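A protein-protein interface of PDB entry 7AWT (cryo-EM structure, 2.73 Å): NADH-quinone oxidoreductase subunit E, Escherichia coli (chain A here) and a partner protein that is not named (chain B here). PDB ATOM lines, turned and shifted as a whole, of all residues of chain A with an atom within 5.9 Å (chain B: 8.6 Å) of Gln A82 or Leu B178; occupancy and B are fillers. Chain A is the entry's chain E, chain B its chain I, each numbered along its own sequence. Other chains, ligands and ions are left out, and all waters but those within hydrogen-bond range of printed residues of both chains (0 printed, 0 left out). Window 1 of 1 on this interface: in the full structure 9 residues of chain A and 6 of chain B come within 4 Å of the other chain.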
ATOM      1  N   GLY A  48     -22.815  -6.052  17.512  1.00  0.00           N
ATOM      2  CA  GLY A  48     -22.340  -4.710  17.262  1.00  0.00           C
ATOM      3  C   GLY A  48     -23.088  -3.961  16.181  1.00  0.00           C
ATOM      4  O   GLY A  48     -22.994  -2.731  16.123  1.00  0.00           O
ATOM      5  N   TRP A  49     -23.822  -4.665  15.325  1.00  0.00           N
ATOM      6  CA  TRP A  49     -24.636  -4.048  14.289  1.00  0.00           C
ATOM      7  C   TRP A  49     -25.631  -5.088  13.802  1.00  0.00           C
ATOM      8  O   TRP A  49     -25.571  -6.257  14.186  1.00  0.00           O
ATOM      9  CB  TRP A  49     -23.780  -3.517  13.141  1.00  0.00           C
ATOM     10  CG  TRP A  49     -22.992  -4.572  12.441  1.00  0.00           C
ATOM     11  CD1 TRP A  49     -21.988  -5.328  12.966  1.00  0.00           C
ATOM     12  CD2 TRP A  49     -23.139  -4.990  11.081  1.00  0.00           C
ATOM     13  NE1 TRP A  49     -21.501  -6.192  12.020  1.00  0.00           N
ATOM     14  CE2 TRP A  49     -22.192  -6.003  10.852  1.00  0.00           C
ATOM     15  CE3 TRP A  49     -23.978  -4.606  10.034  1.00  0.00           C
ATOM     16  CZ2 TRP A  49     -22.062  -6.637   9.623  1.00  0.00           C
ATOM     17  CZ3 TRP A  49     -23.849  -5.234   8.817  1.00  0.00           C
ATOM     18  CH2 TRP A  49     -22.897  -6.237   8.620  1.00  0.00           C
ATOM     19  N   VAL A  50     -26.549  -4.654  12.948  1.00  0.00           N
ATOM     20  CA  VAL A  50     -27.615  -5.535  12.476  1.00  0.00           C
ATOM     21  C   VAL A  50     -27.317  -5.973  11.047  1.00  0.00           C
ATOM     22  O   VAL A  50     -27.501  -5.187  10.107  1.00  0.00           O
ATOM     23  CB  VAL A  50     -28.985  -4.851  12.580  1.00  0.00           C
ATOM     24  CG1 VAL A  50     -30.079  -5.808  12.185  1.00  0.00           C
ATOM     25  CG2 VAL A  50     -29.212  -4.360  13.989  1.00  0.00           C
ATOM     26  N   SER A  77     -31.554   5.990  14.634  1.00  0.00           N
ATOM     27  CA  SER A  77     -30.147   6.250  14.381  1.00  0.00           C
ATOM     28  C   SER A  77     -29.208   5.389  15.211  1.00  0.00           C
ATOM     29  O   SER A  77     -28.011   5.346  14.909  1.00  0.00           O
ATOM     30  CB  SER A  77     -29.832   7.724  14.639  1.00  0.00           C
ATOM     31  OG  SER A  77     -30.324   8.134  15.899  1.00  0.00           O
ATOM     32  N   PHE A  80     -27.642   0.273  14.081  1.00  0.00           N
ATOM     33  CA  PHE A  80     -26.669   0.364  13.003  1.00  0.00           C
ATOM     34  C   PHE A  80     -26.915  -0.727  11.973  1.00  0.00           C
ATOM     35  O   PHE A  80     -27.048  -1.903  12.322  1.00  0.00           O
ATOM     36  CB  PHE A  80     -25.252   0.258  13.556  1.00  0.00           C
ATOM     37  CG  PHE A  80     -24.934   1.290  14.588  1.00  0.00           C
ATOM     38  CD1 PHE A  80     -25.050   2.633  14.295  1.00  0.00           C
ATOM     39  CD2 PHE A  80     -24.525   0.919  15.853  1.00  0.00           C
ATOM     40  CE1 PHE A  80     -24.764   3.583  15.242  1.00  0.00           C
ATOM     41  CE2 PHE A  80     -24.237   1.868  16.801  1.00  0.00           C
ATOM     42  CZ  PHE A  80     -24.356   3.202  16.496  1.00  0.00           C
ATOM     43  N   ARG A  81     -26.943  -0.332  10.719  1.00  0.00           N
ATOM     44  CA  ARG A  81     -27.122  -1.241   9.635  1.00  0.00           C
ATOM     45  C   ARG A  81     -25.902  -1.357   8.745  1.00  0.00           C
ATOM     46  O   ARG A  81     -25.994  -1.851   7.655  1.00  0.00           O
ATOM     47  CB  ARG A  81     -28.338  -0.874   8.851  1.00  0.00           C
ATOM     48  CG  ARG A  81     -29.590  -1.129   9.599  1.00  0.00           C
ATOM     49  CD  ARG A  81     -29.901  -2.577   9.565  1.00  0.00           C
ATOM     50  NE  ARG A  81     -30.442  -2.936   8.292  1.00  0.00           N
ATOM     51  CZ  ARG A  81     -29.849  -3.722   7.428  1.00  0.00           C
ATOM     52  NH1 ARG A  81     -28.694  -4.239   7.700  1.00  0.00           N
ATOM     53  NH2 ARG A  81     -30.421  -3.980   6.288  1.00  0.00           N
ATOM     54  N   GLN A  82     -24.767  -0.883   9.214  1.00  0.00           N
ATOM     55  CA  GLN A  82     -23.504  -0.951   8.503  1.00  0.00           C
ATOM     56  C   GLN A  82     -22.423  -1.369   9.484  1.00  0.00           C
ATOM     57  O   GLN A  82     -22.550  -1.122  10.688  1.00  0.00           O
ATOM     58  CB  GLN A  82     -23.142   0.396   7.861  1.00  0.00           C
ATOM     59  CG  GLN A  82     -23.704   0.569   6.465  1.00  0.00           C
ATOM     60  CD  GLN A  82     -23.178   1.805   5.774  1.00  0.00           C
ATOM     61  OE1 GLN A  82     -22.197   2.404   6.211  1.00  0.00           O
ATOM     62  NE2 GLN A  82     -23.831   2.200   4.692  1.00  0.00           N
ATOM     63  N   PRO A  83     -21.355  -2.009   9.008  1.00  0.00           N
ATOM     64  CA  PRO A  83     -20.329  -2.507   9.931  1.00  0.00           C
ATOM     65  C   PRO A  83     -19.643  -1.396  10.702  1.00  0.00           C
ATOM     66  O   PRO A  83     -18.913  -0.585  10.125  1.00  0.00           O
ATOM     67  CB  PRO A  83     -19.344  -3.229   9.005  1.00  0.00           C
ATOM     68  CG  PRO A  83     -20.123  -3.542   7.787  1.00  0.00           C
ATOM     69  CD  PRO A  83     -21.080  -2.411   7.619  1.00  0.00           C
ATOM     70  N   VAL A  84     -19.807  -1.443  12.016  1.00  0.00           N
ATOM     71  CA  VAL A  84     -19.275  -0.480  12.953  1.00  0.00           C
ATOM     72  C   VAL A  84     -18.255  -1.091  13.879  1.00  0.00           C
ATOM     73  O   VAL A  84     -18.460  -2.161  14.360  1.00  0.00           O
ATOM     74  CB  VAL A  84     -20.389  -0.035  13.846  1.00  0.00           C
ATOM     75  CG1 VAL A  84     -19.841   0.865  14.898  1.00  0.00           C
ATOM     76  CG2 VAL A  84     -21.405   0.691  13.035  1.00  0.00           C
ATOM     77  N   GLY A 118     -18.207   9.273  11.095  1.00  0.00           N
ATOM     78  CA  GLY A 118     -18.923   8.290  10.314  1.00  0.00           C
ATOM     79  C   GLY A 118     -18.097   7.120   9.828  1.00  0.00           C
ATOM     80  O   GLY A 118     -18.617   6.298   9.065  1.00  0.00           O
ATOM     81  N   THR A 127     -15.234   3.561  16.096  1.00  0.00           N
ATOM     82  CA  THR A 127     -16.081   4.318  15.191  1.00  0.00           C
ATOM     83  C   THR A 127     -16.322   5.713  15.768  1.00  0.00           C
ATOM     84  O   THR A 127     -16.264   5.928  16.980  1.00  0.00           O
ATOM     85  CB  THR A 127     -17.407   3.591  14.971  1.00  0.00           C
ATOM     86  OG1 THR A 127     -17.156   2.200  14.755  1.00  0.00           O
ATOM     87  CG2 THR A 127     -18.141   4.149  13.769  1.00  0.00           C
ATOM     88  N   LEU A 129     -19.023   8.994  15.642  1.00  0.00           N
ATOM     89  CA  LEU A 129     -20.342   9.455  15.247  1.00  0.00           C
ATOM     90  C   LEU A 129     -20.725  10.680  16.060  1.00  0.00           C
ATOM     91  O   LEU A 129     -20.303  10.819  17.212  1.00  0.00           O
ATOM     92  CB  LEU A 129     -21.407   8.369  15.453  1.00  0.00           C
ATOM     93  CG  LEU A 129     -21.321   7.112  14.597  1.00  0.00           C
ATOM     94  CD1 LEU A 129     -22.402   6.147  15.008  1.00  0.00           C
ATOM     95  CD2 LEU A 129     -21.458   7.470  13.137  1.00  0.00           C
ATOM     96  N   ILE B 173     -26.752   9.415  -0.421  1.00  0.00           N
ATOM     97  CA  ILE B 173     -26.557   8.884   0.922  1.00  0.00           C
ATOM     98  C   ILE B 173     -27.456   7.670   1.093  1.00  0.00           C
ATOM     99  O   ILE B 173     -28.668   7.748   0.869  1.00  0.00           O
ATOM    100  CB  ILE B 173     -26.866   9.950   1.986  1.00  0.00           C
ATOM    101  CG1 ILE B 173     -25.900  11.124   1.860  1.00  0.00           C
ATOM    102  CG2 ILE B 173     -26.786   9.352   3.373  1.00  0.00           C
ATOM    103  CD1 ILE B 173     -26.161  12.224   2.856  1.00  0.00           C
ATOM    104  N   ASP B 174     -26.865   6.546   1.480  1.00  0.00           N
ATOM    105  CA  ASP B 174     -27.632   5.323   1.636  1.00  0.00           C
ATOM    106  C   ASP B 174     -28.425   5.362   2.934  1.00  0.00           C
ATOM    107  O   ASP B 174     -27.978   5.913   3.942  1.00  0.00           O
ATOM    108  CB  ASP B 174     -26.712   4.105   1.615  1.00  0.00           C
ATOM    109  CG  ASP B 174     -27.462   2.813   1.367  1.00  0.00           C
ATOM    110  OD1 ASP B 174     -28.702   2.863   1.234  1.00  0.00           O
ATOM    111  OD2 ASP B 174     -26.816   1.750   1.298  1.00  0.00           O
ATOM    112  N   VAL B 175     -29.621   4.773   2.900  1.00  0.00           N
ATOM    113  CA  VAL B 175     -30.464   4.782   4.090  1.00  0.00           C
ATOM    114  C   VAL B 175     -29.858   3.930   5.191  1.00  0.00           C
ATOM    115  O   VAL B 175     -30.114   4.163   6.377  1.00  0.00           O
ATOM    116  CB  VAL B 175     -31.890   4.323   3.741  1.00  0.00           C
ATOM    117  CG1 VAL B 175     -32.488   5.256   2.723  1.00  0.00           C
ATOM    118  CG2 VAL B 175     -31.882   2.903   3.215  1.00  0.00           C
ATOM    119  N   LYS B 176     -29.047   2.942   4.833  1.00  0.00           N
ATOM    120  CA  LYS B 176     -28.380   2.106   5.817  1.00  0.00           C
ATOM    121  C   LYS B 176     -27.167   2.779   6.433  1.00  0.00           C
ATOM    122  O   LYS B 176     -26.402   2.110   7.130  1.00  0.00           O
ATOM    123  CB  LYS B 176     -27.962   0.776   5.188  1.00  0.00           C
ATOM    124  CG  LYS B 176     -29.120  -0.144   4.874  1.00  0.00           C
ATOM    125  CD  LYS B 176     -28.775  -1.089   3.744  1.00  0.00           C
ATOM    126  CE  LYS B 176     -27.476  -1.817   4.020  1.00  0.00           C
ATOM    127  NZ  LYS B 176     -27.117  -2.732   2.906  1.00  0.00           N
ATOM    128  N   SER B 177     -26.971   4.072   6.197  1.00  0.00           N
ATOM    129  CA  SER B 177     -25.839   4.770   6.778  1.00  0.00           C
ATOM    130  C   SER B 177     -25.939   4.770   8.302  1.00  0.00           C
ATOM    131  O   SER B 177     -26.957   4.404   8.890  1.00  0.00           O
ATOM    132  CB  SER B 177     -25.764   6.202   6.258  1.00  0.00           C
ATOM    133  OG  SER B 177     -24.464   6.736   6.423  1.00  0.00           O
ATOM    134  N   LEU B 178     -24.835   5.241   8.886  1.00  0.00           N
ATOM    135  CA  LEU B 178     -24.615   5.353  10.316  1.00  0.00           C
ATOM    136  C   LEU B 178     -24.827   6.768  10.796  1.00  0.00           C
ATOM    137  O   LEU B 178     -25.198   6.991  11.937  1.00  0.00           O
ATOM    138  CB  LEU B 178     -23.178   4.976  10.654  1.00  0.00           C
ATOM    139  CG  LEU B 178     -22.726   3.540  10.495  1.00  0.00           C
ATOM    140  CD1 LEU B 178     -21.535   3.305  11.395  1.00  0.00           C
ATOM    141  CD2 LEU B 178     -23.870   2.649  10.901  1.00  0.00           C
ATOM    142  N   LEU B 179     -24.555   7.736   9.938  1.00  0.00           N
ATOM    143  CA  LEU B 179     -24.729   9.128  10.312  1.00  0.00           C
ATOM    144  C   LEU B 179     -26.197   9.426  10.536  1.00  0.00           C
ATOM    145  O   LEU B 179     -27.057   8.889   9.845  1.00  0.00           O
ATOM    146  CB  LEU B 179     -24.141  10.049   9.257  1.00  0.00           C
ATOM    147  CG  LEU B 179     -22.638  10.230   9.407  1.00  0.00           C
ATOM    148  CD1 LEU B 179     -22.096  11.230   8.412  1.00  0.00           C
ATOM    149  CD2 LEU B 179     -22.315  10.659  10.818  1.00  0.00           C
ATOM    150  N   PRO B 180     -26.493  10.278  11.523  1.00  0.00           N
ATOM    151  CA  PRO B 180     -27.842  10.682  11.905  1.00  0.00           C
ATOM    152  C   PRO B 180     -28.363  11.817  11.041  1.00  0.00           C
ATOM    153  O   PRO B 180     -27.608  12.381  10.251  1.00  0.00           O
ATOM    154  CB  PRO B 180     -27.640  11.182  13.316  1.00  0.00           C
ATOM    155  CG  PRO B 180     -26.282  11.759  13.289  1.00  0.00           C
ATOM    156  CD  PRO B 180     -25.479  10.883  12.392  1.00  0.00           C
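The backbone NH of Val A50 lies within hydrogen-bond range of the backbone carbonyl oxygen of Phe A80 (2.9 Å). NH1 of Arg A81 lies within hydrogen-bond range of O of Val A50 (2.8 Å).
CD1 of Phe A80 touches CD2 of Leu B178, at 3.6 Å. Arg A81 touches Lys B176 (C to O, 3.9 Å). Gln A82 touches Lys B176 (CG to O, 3.2 Å). Ser B177 touches Gln A82. Leu B178 touches Gln A82 (CD2 to CB, 3.9 Å). Val A84 touches Leu B178 (CG2 to CD1, 3.1 Å). Leu B178 touches Leu A129 (CB to CD2, 3.9 Å).
Gln A82 touches just these residues of chain B: Lys B176, Ser B177 and Leu B178. Leu B178 touches just these residues of chain A: Phe A80 (3.6 Å), Gln A82 (3.9 Å), Val A84 (3.1 Å) and Leu A129 (3.9 Å). Pro A83 touches none of the printed residues of chain B. Printed residues of chain A within 4 Å of Ser B177: Gln A82 (3.9 Å). Of the printed residues of chain B, Val A84 touches Leu B178 (3.1 Å). Of the printed residues of chain A, Lys B176 touches Arg A81 and Gln A82. Val A50 touches none of the printed residues of chain B. Trp A49 touches none of the printed residues of chain B. The nearest residue of chain A that does not touch Leu B178 is Thr A127 (4.2 Å).
Of the 8 printed residues of chain B, 3 touch a printed residue of chain A. Of the 12 printed residues of chain A, 5 touch a printed residue of chain B. Along chain A the printed residues that touch a printed residue of chain B span positions 80 to 129. Among the printed residues, no Asp or Glu carboxylate lies within 4 Å of a Lys or Arg side-chain nitrogen of the other chain.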
